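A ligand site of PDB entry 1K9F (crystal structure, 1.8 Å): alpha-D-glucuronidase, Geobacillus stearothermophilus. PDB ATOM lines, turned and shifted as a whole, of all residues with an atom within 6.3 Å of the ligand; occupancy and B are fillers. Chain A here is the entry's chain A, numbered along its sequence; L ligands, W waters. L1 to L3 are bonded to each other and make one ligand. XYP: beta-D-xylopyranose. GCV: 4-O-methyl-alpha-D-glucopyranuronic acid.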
ATOM      1  N   TRP A 150     -16.950  26.439 -18.606  1.00  0.00           N
ATOM      2  CA  TRP A 150     -16.777  25.024 -18.297  1.00  0.00           C
ATOM      3  C   TRP A 150     -17.340  24.762 -16.894  1.00  0.00           C
ATOM      4  O   TRP A 150     -16.965  23.808 -16.217  1.00  0.00           O
ATOM      5  CB  TRP A 150     -15.295  24.625 -18.391  1.00  0.00           C
ATOM      6  CG  TRP A 150     -14.834  24.500 -19.832  1.00  0.00           C
ATOM      7  CD1 TRP A 150     -15.572  24.730 -20.953  1.00  0.00           C
ATOM      8  CD2 TRP A 150     -13.531  24.091 -20.296  1.00  0.00           C
ATOM      9  NE1 TRP A 150     -14.818  24.502 -22.087  1.00  0.00           N
ATOM     10  CE2 TRP A 150     -13.564  24.102 -21.707  1.00  0.00           C
ATOM     11  CE3 TRP A 150     -12.347  23.710 -19.646  1.00  0.00           C
ATOM     12  CZ2 TRP A 150     -12.454  23.754 -22.487  1.00  0.00           C
ATOM     13  CZ3 TRP A 150     -11.241  23.366 -20.417  1.00  0.00           C
ATOM     14  CH2 TRP A 150     -11.301  23.399 -21.827  1.00  0.00           C
ATOM     15  N   GLU A 158     -14.656  23.159 -14.379  1.00  0.00           N
ATOM     16  CA  GLU A 158     -13.569  22.337 -14.872  1.00  0.00           C
ATOM     17  C   GLU A 158     -12.466  23.267 -15.370  1.00  0.00           C
ATOM     18  O   GLU A 158     -12.714  24.136 -16.213  1.00  0.00           O
ATOM     19  CB  GLU A 158     -14.052  21.404 -15.995  1.00  0.00           C
ATOM     20  CG  GLU A 158     -12.986  20.441 -16.453  1.00  0.00           C
ATOM     21  CD  GLU A 158     -13.546  19.249 -17.212  1.00  0.00           C
ATOM     22  OE1 GLU A 158     -14.775  19.008 -17.132  1.00  0.00           O
ATOM     23  OE2 GLU A 158     -12.755  18.543 -17.876  1.00  0.00           O
ATOM     24  N   ARG A 159     -11.271  23.087 -14.835  1.00  0.00           N
ATOM     25  CA  ARG A 159     -10.109  23.921 -15.179  1.00  0.00           C
ATOM     26  C   ARG A 159     -10.392  25.369 -14.766  1.00  0.00           C
ATOM     27  O   ARG A 159      -9.985  26.309 -15.452  1.00  0.00           O
ATOM     28  CB  ARG A 159      -9.803  23.846 -16.676  1.00  0.00           C
ATOM     29  CG  ARG A 159      -9.679  22.431 -17.221  1.00  0.00           C
ATOM     30  CD  ARG A 159      -8.705  21.580 -16.404  1.00  0.00           C
ATOM     31  NE  ARG A 159      -8.664  20.207 -16.923  1.00  0.00           N
ATOM     32  CZ  ARG A 159      -7.907  19.238 -16.418  1.00  0.00           C
ATOM     33  NH1 ARG A 159      -7.123  19.466 -15.376  1.00  0.00           N
ATOM     34  NH2 ARG A 159      -7.933  18.027 -16.983  1.00  0.00           N
ATOM     35  N   ASN A 199     -20.521  23.651 -18.905  1.00  0.00           N
ATOM     36  CA  ASN A 199     -19.409  22.810 -19.329  1.00  0.00           C
ATOM     37  C   ASN A 199     -19.677  22.004 -20.609  1.00  0.00           C
ATOM     38  O   ASN A 199     -20.759  21.427 -20.770  1.00  0.00           O
ATOM     39  CB  ASN A 199     -19.074  21.851 -18.191  1.00  0.00           C
ATOM     40  CG  ASN A 199     -17.704  21.209 -18.325  1.00  0.00           C
ATOM     41  OD1 ASN A 199     -17.069  21.282 -19.380  1.00  0.00           O
ATOM     42  ND2 ASN A 199     -17.248  20.569 -17.262  1.00  0.00           N
ATOM     43  N   VAL A 200     -18.690  21.960 -21.503  1.00  0.00           N
ATOM     44  CA  VAL A 200     -18.832  21.199 -22.738  1.00  0.00           C
ATOM     45  C   VAL A 200     -18.931  19.714 -22.372  1.00  0.00           C
ATOM     46  O   VAL A 200     -19.447  18.908 -23.152  1.00  0.00           O
ATOM     47  CB  VAL A 200     -17.659  21.452 -23.692  1.00  0.00           C
ATOM     48  CG1 VAL A 200     -17.692  22.909 -24.162  1.00  0.00           C
ATOM     49  CG2 VAL A 200     -16.333  21.155 -23.009  1.00  0.00           C
ATOM     50  N   ASN A 201     -18.414  19.348 -21.199  1.00  0.00           N
ATOM     51  CA  ASN A 201     -18.525  17.978 -20.714  1.00  0.00           C
ATOM     52  C   ASN A 201     -19.830  18.039 -19.918  1.00  0.00           C
ATOM     53  O   ASN A 201     -19.825  18.414 -18.738  1.00  0.00           O
ATOM     54  CB  ASN A 201     -17.381  17.597 -19.772  1.00  0.00           C
ATOM     55  CG  ASN A 201     -16.080  17.340 -20.512  1.00  0.00           C
ATOM     56  OD1 ASN A 201     -16.065  16.707 -21.561  1.00  0.00           O
ATOM     57  ND2 ASN A 201     -14.979  17.833 -19.946  1.00  0.00           N
ATOM     58  N   LYS A 281     -19.713  18.647 -27.785  1.00  0.00           N
ATOM     59  CA  LYS A 281     -18.493  17.878 -27.661  1.00  0.00           C
ATOM     60  C   LYS A 281     -18.977  16.438 -27.770  1.00  0.00           C
ATOM     61  O   LYS A 281     -19.581  15.901 -26.837  1.00  0.00           O
ATOM     62  CB  LYS A 281     -17.805  18.089 -26.308  1.00  0.00           C
ATOM     63  CG  LYS A 281     -16.580  17.217 -26.122  1.00  0.00           C
ATOM     64  CD  LYS A 281     -15.890  17.441 -24.785  1.00  0.00           C
ATOM     65  CE  LYS A 281     -14.761  16.448 -24.582  1.00  0.00           C
ATOM     66  NZ  LYS A 281     -14.056  16.656 -23.280  1.00  0.00           N
ATOM     67  N   ARG A 318     -17.368  21.084 -31.780  1.00  0.00           N
ATOM     68  CA  ARG A 318     -15.950  21.101 -31.445  1.00  0.00           C
ATOM     69  C   ARG A 318     -15.182  20.006 -32.184  1.00  0.00           C
ATOM     70  O   ARG A 318     -15.609  18.848 -32.211  1.00  0.00           O
ATOM     71  CB  ARG A 318     -15.764  20.940 -29.931  1.00  0.00           C
ATOM     72  CG  ARG A 318     -16.347  22.088 -29.136  1.00  0.00           C
ATOM     73  CD  ARG A 318     -16.087  21.920 -27.646  1.00  0.00           C
ATOM     74  NE  ARG A 318     -14.737  22.313 -27.245  1.00  0.00           N
ATOM     75  CZ  ARG A 318     -13.939  21.563 -26.493  1.00  0.00           C
ATOM     76  NH1 ARG A 318     -14.340  20.373 -26.077  1.00  0.00           N
ATOM     77  NH2 ARG A 318     -12.742  22.016 -26.129  1.00  0.00           N
ATOM     78  N   PHE A 320     -12.291  18.950 -31.386  1.00  0.00           N
ATOM     79  CA  PHE A 320     -11.317  18.373 -30.474  1.00  0.00           C
ATOM     80  C   PHE A 320     -11.610  16.881 -30.403  1.00  0.00           C
ATOM     81  O   PHE A 320     -12.145  16.380 -29.409  1.00  0.00           O
ATOM     82  CB  PHE A 320     -11.439  19.001 -29.088  1.00  0.00           C
ATOM     83  CG  PHE A 320     -10.318  18.637 -28.153  1.00  0.00           C
ATOM     84  CD1 PHE A 320      -9.014  19.046 -28.423  1.00  0.00           C
ATOM     85  CD2 PHE A 320     -10.560  17.905 -26.994  1.00  0.00           C
ATOM     86  CE1 PHE A 320      -7.965  18.728 -27.565  1.00  0.00           C
ATOM     87  CE2 PHE A 320      -9.514  17.582 -26.123  1.00  0.00           C
ATOM     88  CZ  PHE A 320      -8.217  17.993 -26.408  1.00  0.00           C
ATOM     89  N   TYR A 322      -9.868  12.979 -31.190  1.00  0.00           N
ATOM     90  CA  TYR A 322      -8.663  12.196 -31.446  1.00  0.00           C
ATOM     91  C   TYR A 322      -8.759  10.869 -30.702  1.00  0.00           C
ATOM     92  O   TYR A 322      -9.725  10.610 -29.988  1.00  0.00           O
ATOM     93  CB  TYR A 322      -7.427  12.960 -30.963  1.00  0.00           C
ATOM     94  CG  TYR A 322      -7.447  13.260 -29.484  1.00  0.00           C
ATOM     95  CD1 TYR A 322      -8.243  14.282 -28.973  1.00  0.00           C
ATOM     96  CD2 TYR A 322      -6.705  12.493 -28.582  1.00  0.00           C
ATOM     97  CE1 TYR A 322      -8.296  14.549 -27.600  1.00  0.00           C
ATOM     98  CE2 TYR A 322      -6.744  12.749 -27.209  1.00  0.00           C
ATOM     99  CZ  TYR A 322      -7.543  13.778 -26.726  1.00  0.00           C
ATOM    100  OH  TYR A 322      -7.586  14.033 -25.379  1.00  0.00           O
ATOM    101  N   ARG A 335      -1.353  12.214 -32.783  1.00  0.00           N
ATOM    102  CA  ARG A 335      -2.540  12.920 -32.327  1.00  0.00           C
ATOM    103  C   ARG A 335      -2.700  14.272 -33.029  1.00  0.00           C
ATOM    104  O   ARG A 335      -3.821  14.720 -33.289  1.00  0.00           O
ATOM    105  CB  ARG A 335      -2.486  13.115 -30.802  1.00  0.00           C
ATOM    106  CG  ARG A 335      -3.560  14.042 -30.259  1.00  0.00           C
ATOM    107  CD  ARG A 335      -3.512  14.098 -28.741  1.00  0.00           C
ATOM    108  NE  ARG A 335      -4.383  15.135 -28.210  1.00  0.00           N
ATOM    109  CZ  ARG A 335      -4.606  15.324 -26.921  1.00  0.00           C
ATOM    110  NH1 ARG A 335      -4.034  14.545 -26.016  1.00  0.00           N
ATOM    111  NH2 ARG A 335      -5.417  16.298 -26.524  1.00  0.00           N
ATOM    112  N   LYS A 359      -9.480  24.320 -31.803  1.00  0.00           N
ATOM    113  CA  LYS A 359      -8.538  24.975 -30.895  1.00  0.00           C
ATOM    114  C   LYS A 359      -7.429  25.631 -31.712  1.00  0.00           C
ATOM    115  O   LYS A 359      -7.167  25.207 -32.849  1.00  0.00           O
ATOM    116  CB  LYS A 359      -7.948  23.959 -29.905  1.00  0.00           C
ATOM    117  CG  LYS A 359      -8.970  23.401 -28.930  1.00  0.00           C
ATOM    118  CD  LYS A 359      -8.346  22.533 -27.852  1.00  0.00           C
ATOM    119  CE  LYS A 359      -9.398  22.066 -26.850  1.00  0.00           C
ATOM    120  NZ  LYS A 359      -8.793  21.301 -25.723  1.00  0.00           N
ATOM    121  N   MET A 363      -3.092  20.116 -30.674  1.00  0.00           N
ATOM    122  CA  MET A 363      -2.949  19.247 -29.508  1.00  0.00           C
ATOM    123  C   MET A 363      -3.901  19.654 -28.391  1.00  0.00           C
ATOM    124  O   MET A 363      -5.049  19.223 -28.387  1.00  0.00           O
ATOM    125  CB  MET A 363      -1.498  19.248 -29.031  1.00  0.00           C
ATOM    126  CG  MET A 363      -0.526  18.574 -30.012  1.00  0.00           C
ATOM    127  SD  MET A 363      -0.886  16.809 -30.269  1.00  0.00           S
ATOM    128  CE  MET A 363      -0.110  16.102 -28.810  1.00  0.00           C
ATOM    129  N   ASP A 364      -3.455  20.491 -27.452  1.00  0.00           N
ATOM    130  CA  ASP A 364      -4.352  20.896 -26.369  1.00  0.00           C
ATOM    131  C   ASP A 364      -3.925  22.109 -25.547  1.00  0.00           C
ATOM    132  O   ASP A 364      -3.461  21.969 -24.410  1.00  0.00           O
ATOM    133  CB  ASP A 364      -4.616  19.706 -25.442  1.00  0.00           C
ATOM    134  CG  ASP A 364      -5.582  20.047 -24.299  1.00  0.00           C
ATOM    135  OD1 ASP A 364      -6.414  20.967 -24.469  1.00  0.00           O
ATOM    136  OD2 ASP A 364      -5.504  19.375 -23.243  1.00  0.00           O
ATOM    137  N   PHE A 365      -4.069  23.285 -26.134  1.00  0.00           N
ATOM    138  CA  PHE A 365      -3.758  24.541 -25.454  1.00  0.00           C
ATOM    139  C   PHE A 365      -2.418  24.603 -24.710  1.00  0.00           C
ATOM    140  O   PHE A 365      -2.354  25.163 -23.616  1.00  0.00           O
ATOM    141  CB  PHE A 365      -4.864  24.883 -24.444  1.00  0.00           C
ATOM    142  CG  PHE A 365      -6.233  25.025 -25.049  1.00  0.00           C
ATOM    143  CD1 PHE A 365      -6.430  25.805 -26.184  1.00  0.00           C
ATOM    144  CD2 PHE A 365      -7.343  24.460 -24.429  1.00  0.00           C
ATOM    145  CE1 PHE A 365      -7.721  26.028 -26.686  1.00  0.00           C
ATOM    146  CE2 PHE A 365      -8.633  24.665 -24.922  1.00  0.00           C
ATOM    147  CZ  PHE A 365      -8.816  25.462 -26.048  1.00  0.00           C
ATOM    148  N   GLU A 386     -11.125  28.273 -31.152  1.00  0.00           N
ATOM    149  CA  GLU A 386     -11.340  28.216 -29.707  1.00  0.00           C
ATOM    150  C   GLU A 386      -9.997  28.446 -29.029  1.00  0.00           C
ATOM    151  O   GLU A 386      -9.024  27.773 -29.345  1.00  0.00           O
ATOM    152  CB  GLU A 386     -11.873  26.839 -29.308  1.00  0.00           C
ATOM    153  CG  GLU A 386     -12.184  26.702 -27.807  1.00  0.00           C
ATOM    154  CD  GLU A 386     -12.601  25.297 -27.415  1.00  0.00           C
ATOM    155  OE1 GLU A 386     -13.280  24.623 -28.222  1.00  0.00           O
ATOM    156  OE2 GLU A 386     -12.269  24.869 -26.293  1.00  0.00           O
ATOM    157  N   GLN A 388      -8.088  29.328 -25.072  1.00  0.00           N
ATOM    158  CA  GLN A 388      -8.358  29.101 -23.666  1.00  0.00           C
ATOM    159  C   GLN A 388      -7.912  30.261 -22.798  1.00  0.00           C
ATOM    160  O   GLN A 388      -6.719  30.492 -22.626  1.00  0.00           O
ATOM    161  CB  GLN A 388      -7.683  27.790 -23.224  1.00  0.00           C
ATOM    162  CG  GLN A 388      -8.147  27.274 -21.871  1.00  0.00           C
ATOM    163  CD  GLN A 388      -7.450  25.986 -21.478  1.00  0.00           C
ATOM    164  OE1 GLN A 388      -6.227  25.873 -21.546  1.00  0.00           O
ATOM    165  NE2 GLN A 388      -8.240  25.010 -21.048  1.00  0.00           N
ATOM    166  N   GLU A 392      -5.060  26.769 -18.073  1.00  0.00           N
ATOM    167  CA  GLU A 392      -4.836  25.370 -17.738  1.00  0.00           C
ATOM    168  C   GLU A 392      -3.381  24.944 -17.794  1.00  0.00           C
ATOM    169  O   GLU A 392      -2.850  24.386 -16.822  1.00  0.00           O
ATOM    170  CB  GLU A 392      -5.659  24.445 -18.644  1.00  0.00           C
ATOM    171  CG  GLU A 392      -5.454  22.968 -18.327  1.00  0.00           C
ATOM    172  CD  GLU A 392      -6.386  22.062 -19.111  1.00  0.00           C
ATOM    173  OE1 GLU A 392      -7.198  22.574 -19.910  1.00  0.00           O
ATOM    174  OE2 GLU A 392      -6.293  20.827 -18.923  1.00  0.00           O
ATOM    175  N   TYR A 393      -2.720  25.185 -18.919  1.00  0.00           N
ATOM    176  CA  TYR A 393      -1.328  24.810 -19.086  1.00  0.00           C
ATOM    177  C   TYR A 393      -0.417  26.032 -19.069  1.00  0.00           C
ATOM    178  O   TYR A 393       0.777  25.926 -19.320  1.00  0.00           O
ATOM    179  CB  TYR A 393      -1.134  24.063 -20.407  1.00  0.00           C
ATOM    180  CG  TYR A 393      -1.959  22.797 -20.521  1.00  0.00           C
ATOM    181  CD1 TYR A 393      -1.566  21.626 -19.875  1.00  0.00           C
ATOM    182  CD2 TYR A 393      -3.107  22.769 -21.317  1.00  0.00           C
ATOM    183  CE1 TYR A 393      -2.310  20.447 -20.007  1.00  0.00           C
ATOM    184  CE2 TYR A 393      -3.852  21.599 -21.453  1.00  0.00           C
ATOM    185  CZ  TYR A 393      -3.441  20.441 -20.805  1.00  0.00           C
ATOM    186  OH  TYR A 393      -4.172  19.269 -20.947  1.00  0.00           O
ATOM    187  N   TRP A 520       3.668  20.019 -23.067  1.00  0.00           N
ATOM    188  CA  TRP A 520       3.445  19.134 -21.922  1.00  0.00           C
ATOM    189  C   TRP A 520       4.480  19.197 -20.800  1.00  0.00           C
ATOM    190  O   TRP A 520       4.804  20.271 -20.325  1.00  0.00           O
ATOM    191  CB  TRP A 520       3.240  17.701 -22.435  1.00  0.00           C
ATOM    192  CG  TRP A 520       2.192  17.682 -23.514  1.00  0.00           C
ATOM    193  CD1 TRP A 520       2.393  17.844 -24.860  1.00  0.00           C
ATOM    194  CD2 TRP A 520       0.772  17.694 -23.328  1.00  0.00           C
ATOM    195  NE1 TRP A 520       1.187  17.954 -25.509  1.00  0.00           N
ATOM    196  CE2 TRP A 520       0.180  17.870 -24.598  1.00  0.00           C
ATOM    197  CE3 TRP A 520      -0.061  17.578 -22.196  1.00  0.00           C
ATOM    198  CZ2 TRP A 520      -1.212  17.937 -24.772  1.00  0.00           C
ATOM    199  CZ3 TRP A 520      -1.440  17.644 -22.375  1.00  0.00           C
ATOM    200  CH2 TRP A 520      -2.006  17.816 -23.656  1.00  0.00           C
ATOM    201  N   PRO A 524       0.230  14.944 -14.437  1.00  0.00           N
ATOM    202  CA  PRO A 524      -1.014  14.419 -15.002  1.00  0.00           C
ATOM    203  C   PRO A 524      -2.213  14.795 -14.132  1.00  0.00           C
ATOM    204  O   PRO A 524      -2.070  15.065 -12.937  1.00  0.00           O
ATOM    205  CB  PRO A 524      -0.780  12.912 -15.016  1.00  0.00           C
ATOM    206  CG  PRO A 524       0.717  12.787 -15.125  1.00  0.00           C
ATOM    207  CD  PRO A 524       1.192  13.854 -14.177  1.00  0.00           C
ATOM    208  N   GLY A 525      -3.391  14.825 -14.743  1.00  0.00           N
ATOM    209  CA  GLY A 525      -4.584  15.153 -13.990  1.00  0.00           C
ATOM    210  C   GLY A 525      -4.865  16.635 -13.842  1.00  0.00           C
ATOM    211  O   GLY A 525      -5.614  17.189 -14.634  1.00  0.00           O
ATOM    212  N   HIS A 526      -4.276  17.263 -12.825  1.00  0.00           N
ATOM    213  CA  HIS A 526      -4.503  18.686 -12.602  1.00  0.00           C
ATOM    214  C   HIS A 526      -3.685  19.589 -13.533  1.00  0.00           C
ATOM    215  O   HIS A 526      -3.959  20.775 -13.658  1.00  0.00           O
ATOM    216  CB  HIS A 526      -4.233  19.048 -11.133  1.00  0.00           C
ATOM    217  CG  HIS A 526      -2.822  18.822 -10.698  1.00  0.00           C
ATOM    218  ND1 HIS A 526      -2.449  17.780  -9.884  1.00  0.00           N
ATOM    219  CD2 HIS A 526      -1.697  19.536 -10.940  1.00  0.00           C
ATOM    220  CE1 HIS A 526      -1.155  17.853  -9.641  1.00  0.00           C
ATOM    221  NE2 HIS A 526      -0.676  18.907 -10.268  1.00  0.00           N
ATOM    222  N   HIS A 527      -2.674  19.011 -14.174  1.00  0.00           N
ATOM    223  CA  HIS A 527      -1.844  19.709 -15.157  1.00  0.00           C
ATOM    224  C   HIS A 527      -1.015  20.903 -14.698  1.00  0.00           C
ATOM    225  O   HIS A 527      -0.562  21.698 -15.522  1.00  0.00           O
ATOM    226  CB  HIS A 527      -2.735  20.141 -16.322  1.00  0.00           C
ATOM    227  CG  HIS A 527      -3.385  18.990 -17.032  1.00  0.00           C
ATOM    228  ND1 HIS A 527      -4.481  19.143 -17.856  1.00  0.00           N
ATOM    229  CD2 HIS A 527      -3.082  17.673 -17.035  1.00  0.00           C
ATOM    230  CE1 HIS A 527      -4.831  17.961 -18.338  1.00  0.00           C
ATOM    231  NE2 HIS A 527      -3.993  17.051 -17.861  1.00  0.00           N
ATOM    232  N   TYR A 535       3.035  12.334 -18.875  1.00  0.00           N
ATOM    233  CA  TYR A 535       2.185  11.612 -19.818  1.00  0.00           C
ATOM    234  C   TYR A 535       3.001  10.886 -20.878  1.00  0.00           C
ATOM    235  O   TYR A 535       2.444  10.391 -21.861  1.00  0.00           O
ATOM    236  CB  TYR A 535       1.240  12.601 -20.522  1.00  0.00           C
ATOM    237  CG  TYR A 535       0.055  13.084 -19.708  1.00  0.00           C
ATOM    238  CD1 TYR A 535      -0.946  12.207 -19.298  1.00  0.00           C
ATOM    239  CD2 TYR A 535      -0.088  14.437 -19.392  1.00  0.00           C
ATOM    240  CE1 TYR A 535      -2.052  12.649 -18.598  1.00  0.00           C
ATOM    241  CE2 TYR A 535      -1.199  14.893 -18.688  1.00  0.00           C
ATOM    242  CZ  TYR A 535      -2.179  13.997 -18.295  1.00  0.00           C
ATOM    243  OH  TYR A 535      -3.287  14.429 -17.615  1.00  0.00           O
ATOM    244  N   TRP A 540      -2.505   9.148 -24.138  1.00  0.00           N
ATOM    245  CA  TRP A 540      -3.026  10.409 -24.655  1.00  0.00           C
ATOM    246  C   TRP A 540      -2.325  10.955 -25.895  1.00  0.00           C
ATOM    247  O   TRP A 540      -2.711  12.004 -26.408  1.00  0.00           O
ATOM    248  CB  TRP A 540      -3.026  11.478 -23.570  1.00  0.00           C
ATOM    249  CG  TRP A 540      -3.949  11.182 -22.426  1.00  0.00           C
ATOM    250  CD1 TRP A 540      -3.609  10.680 -21.206  1.00  0.00           C
ATOM    251  CD2 TRP A 540      -5.371  11.372 -22.398  1.00  0.00           C
ATOM    252  NE1 TRP A 540      -4.726  10.549 -20.417  1.00  0.00           N
ATOM    253  CE2 TRP A 540      -5.815  10.973 -21.128  1.00  0.00           C
ATOM    254  CE3 TRP A 540      -6.305  11.852 -23.331  1.00  0.00           C
ATOM    255  CZ2 TRP A 540      -7.166  11.029 -20.755  1.00  0.00           C
ATOM    256  CZ3 TRP A 540      -7.643  11.906 -22.963  1.00  0.00           C
ATOM    257  CH2 TRP A 540      -8.067  11.494 -21.678  1.00  0.00           C
ATOM    258  N   THR A 542       0.648  12.285 -26.210  1.00  0.00           N
ATOM    259  CA  THR A 542       1.403  13.494 -25.933  1.00  0.00           C
ATOM    260  C   THR A 542       2.799  13.096 -25.458  1.00  0.00           C
ATOM    261  O   THR A 542       3.053  13.020 -24.252  1.00  0.00           O
ATOM    262  CB  THR A 542       0.695  14.327 -24.853  1.00  0.00           C
ATOM    263  OG1 THR A 542       0.565  13.539 -23.666  1.00  0.00           O
ATOM    264  CG2 THR A 542      -0.681  14.729 -25.322  1.00  0.00           C
HETATM  265  O1  XYP L   1     -11.395  12.368 -16.974  1.00  0.00           O
HETATM  266  C1  XYP L   1     -10.811  13.510 -17.489  1.00  0.00           C
HETATM  267  C2  XYP L   1      -9.498  13.817 -16.743  1.00  0.00           C
HETATM  268  C3  XYP L   1      -8.779  15.000 -17.374  1.00  0.00           C
HETATM  269  C4  XYP L   1      -8.618  14.768 -18.871  1.00  0.00           C
HETATM  270  C5  XYP L   1      -9.974  14.454 -19.514  1.00  0.00           C
HETATM  271  O2  XYP L   1      -9.792  14.116 -15.383  1.00  0.00           O
HETATM  272  O3  XYP L   1      -7.498  15.158 -16.785  1.00  0.00           O
HETATM  273  O4  XYP L   1      -8.039  15.914 -19.510  1.00  0.00           O
HETATM  274  O5  XYP L   1     -10.549  13.295 -18.880  1.00  0.00           O
HETATM  275  C1  XYP L   2      -7.180  15.585 -20.526  1.00  0.00           C
HETATM  276  C2  XYP L   2      -7.086  16.700 -21.575  1.00  0.00           C
HETATM  277  C3  XYP L   2      -6.265  16.082 -22.733  1.00  0.00           C
HETATM  278  C4  XYP L   2      -4.866  15.674 -22.191  1.00  0.00           C
HETATM  279  C5  XYP L   2      -4.981  14.761 -20.962  1.00  0.00           C
HETATM  280  O2  XYP L   2      -8.426  17.107 -21.995  1.00  0.00           O
HETATM  281  O3  XYP L   2      -6.119  17.002 -23.797  1.00  0.00           O
HETATM  282  O4  XYP L   2      -4.105  15.015 -23.200  1.00  0.00           O
HETATM  283  O5  XYP L   2      -5.874  15.330 -19.979  1.00  0.00           O
HETATM  284  C7  GCV L   3     -13.708  20.292 -20.623  1.00  0.00           C
HETATM  285  C1  GCV L   3      -8.650  18.485 -22.083  1.00  0.00           C
HETATM  286  C2  GCV L   3      -8.878  19.175 -20.714  1.00  0.00           C
HETATM  287  C3  GCV L   3     -10.445  19.031 -20.459  1.00  0.00           C
HETATM  288  C4  GCV L   3     -11.418  19.529 -21.417  1.00  0.00           C
HETATM  289  C5  GCV L   3     -10.777  19.210 -22.735  1.00  0.00           C
HETATM  290  C6  GCV L   3     -11.579  19.561 -23.918  1.00  0.00           C
HETATM  291  O2  GCV L   3      -7.776  18.933 -19.845  1.00  0.00           O
HETATM  292  O3  GCV L   3     -10.462  19.639 -19.149  1.00  0.00           O
HETATM  293  O4  GCV L   3     -12.851  19.436 -21.413  1.00  0.00           O
HETATM  294  O5  GCV L   3      -9.449  18.797 -23.210  1.00  0.00           O
HETATM  295  O6A GCV L   3     -11.053  20.573 -24.658  1.00  0.00           O
HETATM  296  O6B GCV L   3     -12.714  18.821 -24.059  1.00  0.00           O
HETATM  297  O   HOH W   1      -5.381  12.806 -17.075  1.00  0.00           O
HETATM  298  O   HOH W   2      -1.850  14.193 -22.137  1.00  0.00           O
HETATM  299  O   HOH W   3      -8.155  21.800 -22.422  1.00  0.00           O
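NE of Arg 159 is in salt-bridge range of OE2 of Glu 392, at 3.2 Å.
The side-chain carboxylate (OE2) of Glu 392 is in hydrogen-bond range of a ring nitrogen (ND1) of His 527, at 2.7 Å.
The side-chain amino group (NZ) of Lys 281 lies within hydrogen-bond range of the side-chain amide oxygen (OD1) of Asn 201 (2.6 Å).
The side-chain carboxylate of Glu 386 is in salt-bridge range of the guanidinium group of Arg 318 (2.9 Å).
The side-chain carboxylate (OE1) of Glu 158 sits at hydrogen-bond distance from the side-chain amide nitrogen (ND2) of Asn 201 (3.1 Å).
The backbone NH (N) of Glu 158 lies within hydrogen-bond range of the backbone carbonyl oxygen (O) of Trp 150.
The guanidinium group (NH1) of Arg 159 sits at hydrogen-bond distance from the backbone carbonyl oxygen (O) of Gly 525, at 2.8 Å.
The backbone carbonyl oxygen (O) of Trp 150 sits at hydrogen-bond distance from the side-chain amide nitrogen (ND2) of Asn 199, 3.4 Å away.
Trp 150 touches the ligand.
Asn 199 touches the ligand.
Val 200 touches the ligand.
CE2 of Phe 320 touches O5 of GCV L3 (3.2 Å).
Tyr 322 touches the ligand.
OH of Tyr 393 touches O2 of GCV L3 (3.8 Å).
CH2 of Trp 520 touches O4 of XYP L2 (3.5 Å).
Gly 525 touches the ligand.
OH of Tyr 535 touches O5 of XYP L2, 3.6 Å away.
CD2 of Trp 540 touches C5 of XYP L2, 3.7 Å away.
Within 4 Å of the ligand: Trp 150, Glu 158, Arg 159, Asn 199, Val 200, Asn 201, Lys 281, Arg 318, Phe 320, Tyr 322, Arg 335, Lys 359, Asp 364, Glu 392, Tyr 393, Trp 520, Gly 525, His 527, Tyr 535 and Trp 540.
The nearest printed residue that does not touch the ligand is Thr 542 (4.04 Å).
The side-chain carboxylate (OD2) of Asp 364 lies within hydrogen-bond range of an oxygen (O3) of XYP L2 (2.5 Å).
OE2 of Glu 392 lies within hydrogen-bond range of O2 of GCV L3, at 2.6 Å.
O6A of GCV L3 is in salt-bridge range of NZ of Lys 359, 2.6 Å away.
O6B of GCV L3 is in salt-bridge range of NZ of Lys 281 (2.7 Å).
The guanidinium group (NH2) of Arg 318 is in salt-bridge range of an oxygen (O6A) of GCV L3 (2.7 Å).
OE2 of Glu 158 is in hydrogen-bond range of O3 of GCV L3 (2.8 Å).
ND2 of Asn 201 sits close to O4 of GCV L3 (3.0 Å).
NH1 of Arg 335 sits at hydrogen-bond distance from O4 of XYP L2 (2.9 Å).
The guanidinium group (NH2) of Arg 159 sits at hydrogen-bond distance from an oxygen (O3) of XYP L1 (2.9 Å).
NE2 of His 527 sits close to O5 of XYP L2 (3.3 Å).
Water W2 bridges an oxygen (O4) of XYP L2 (2.6 Å) and the side-chain hydroxyl of Thr 542 (2.9 Å).
Water W1 lies within hydrogen-bond range of OH of Tyr 535 (2.7 Å) and O3 of XYP L1 (3.2 Å).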
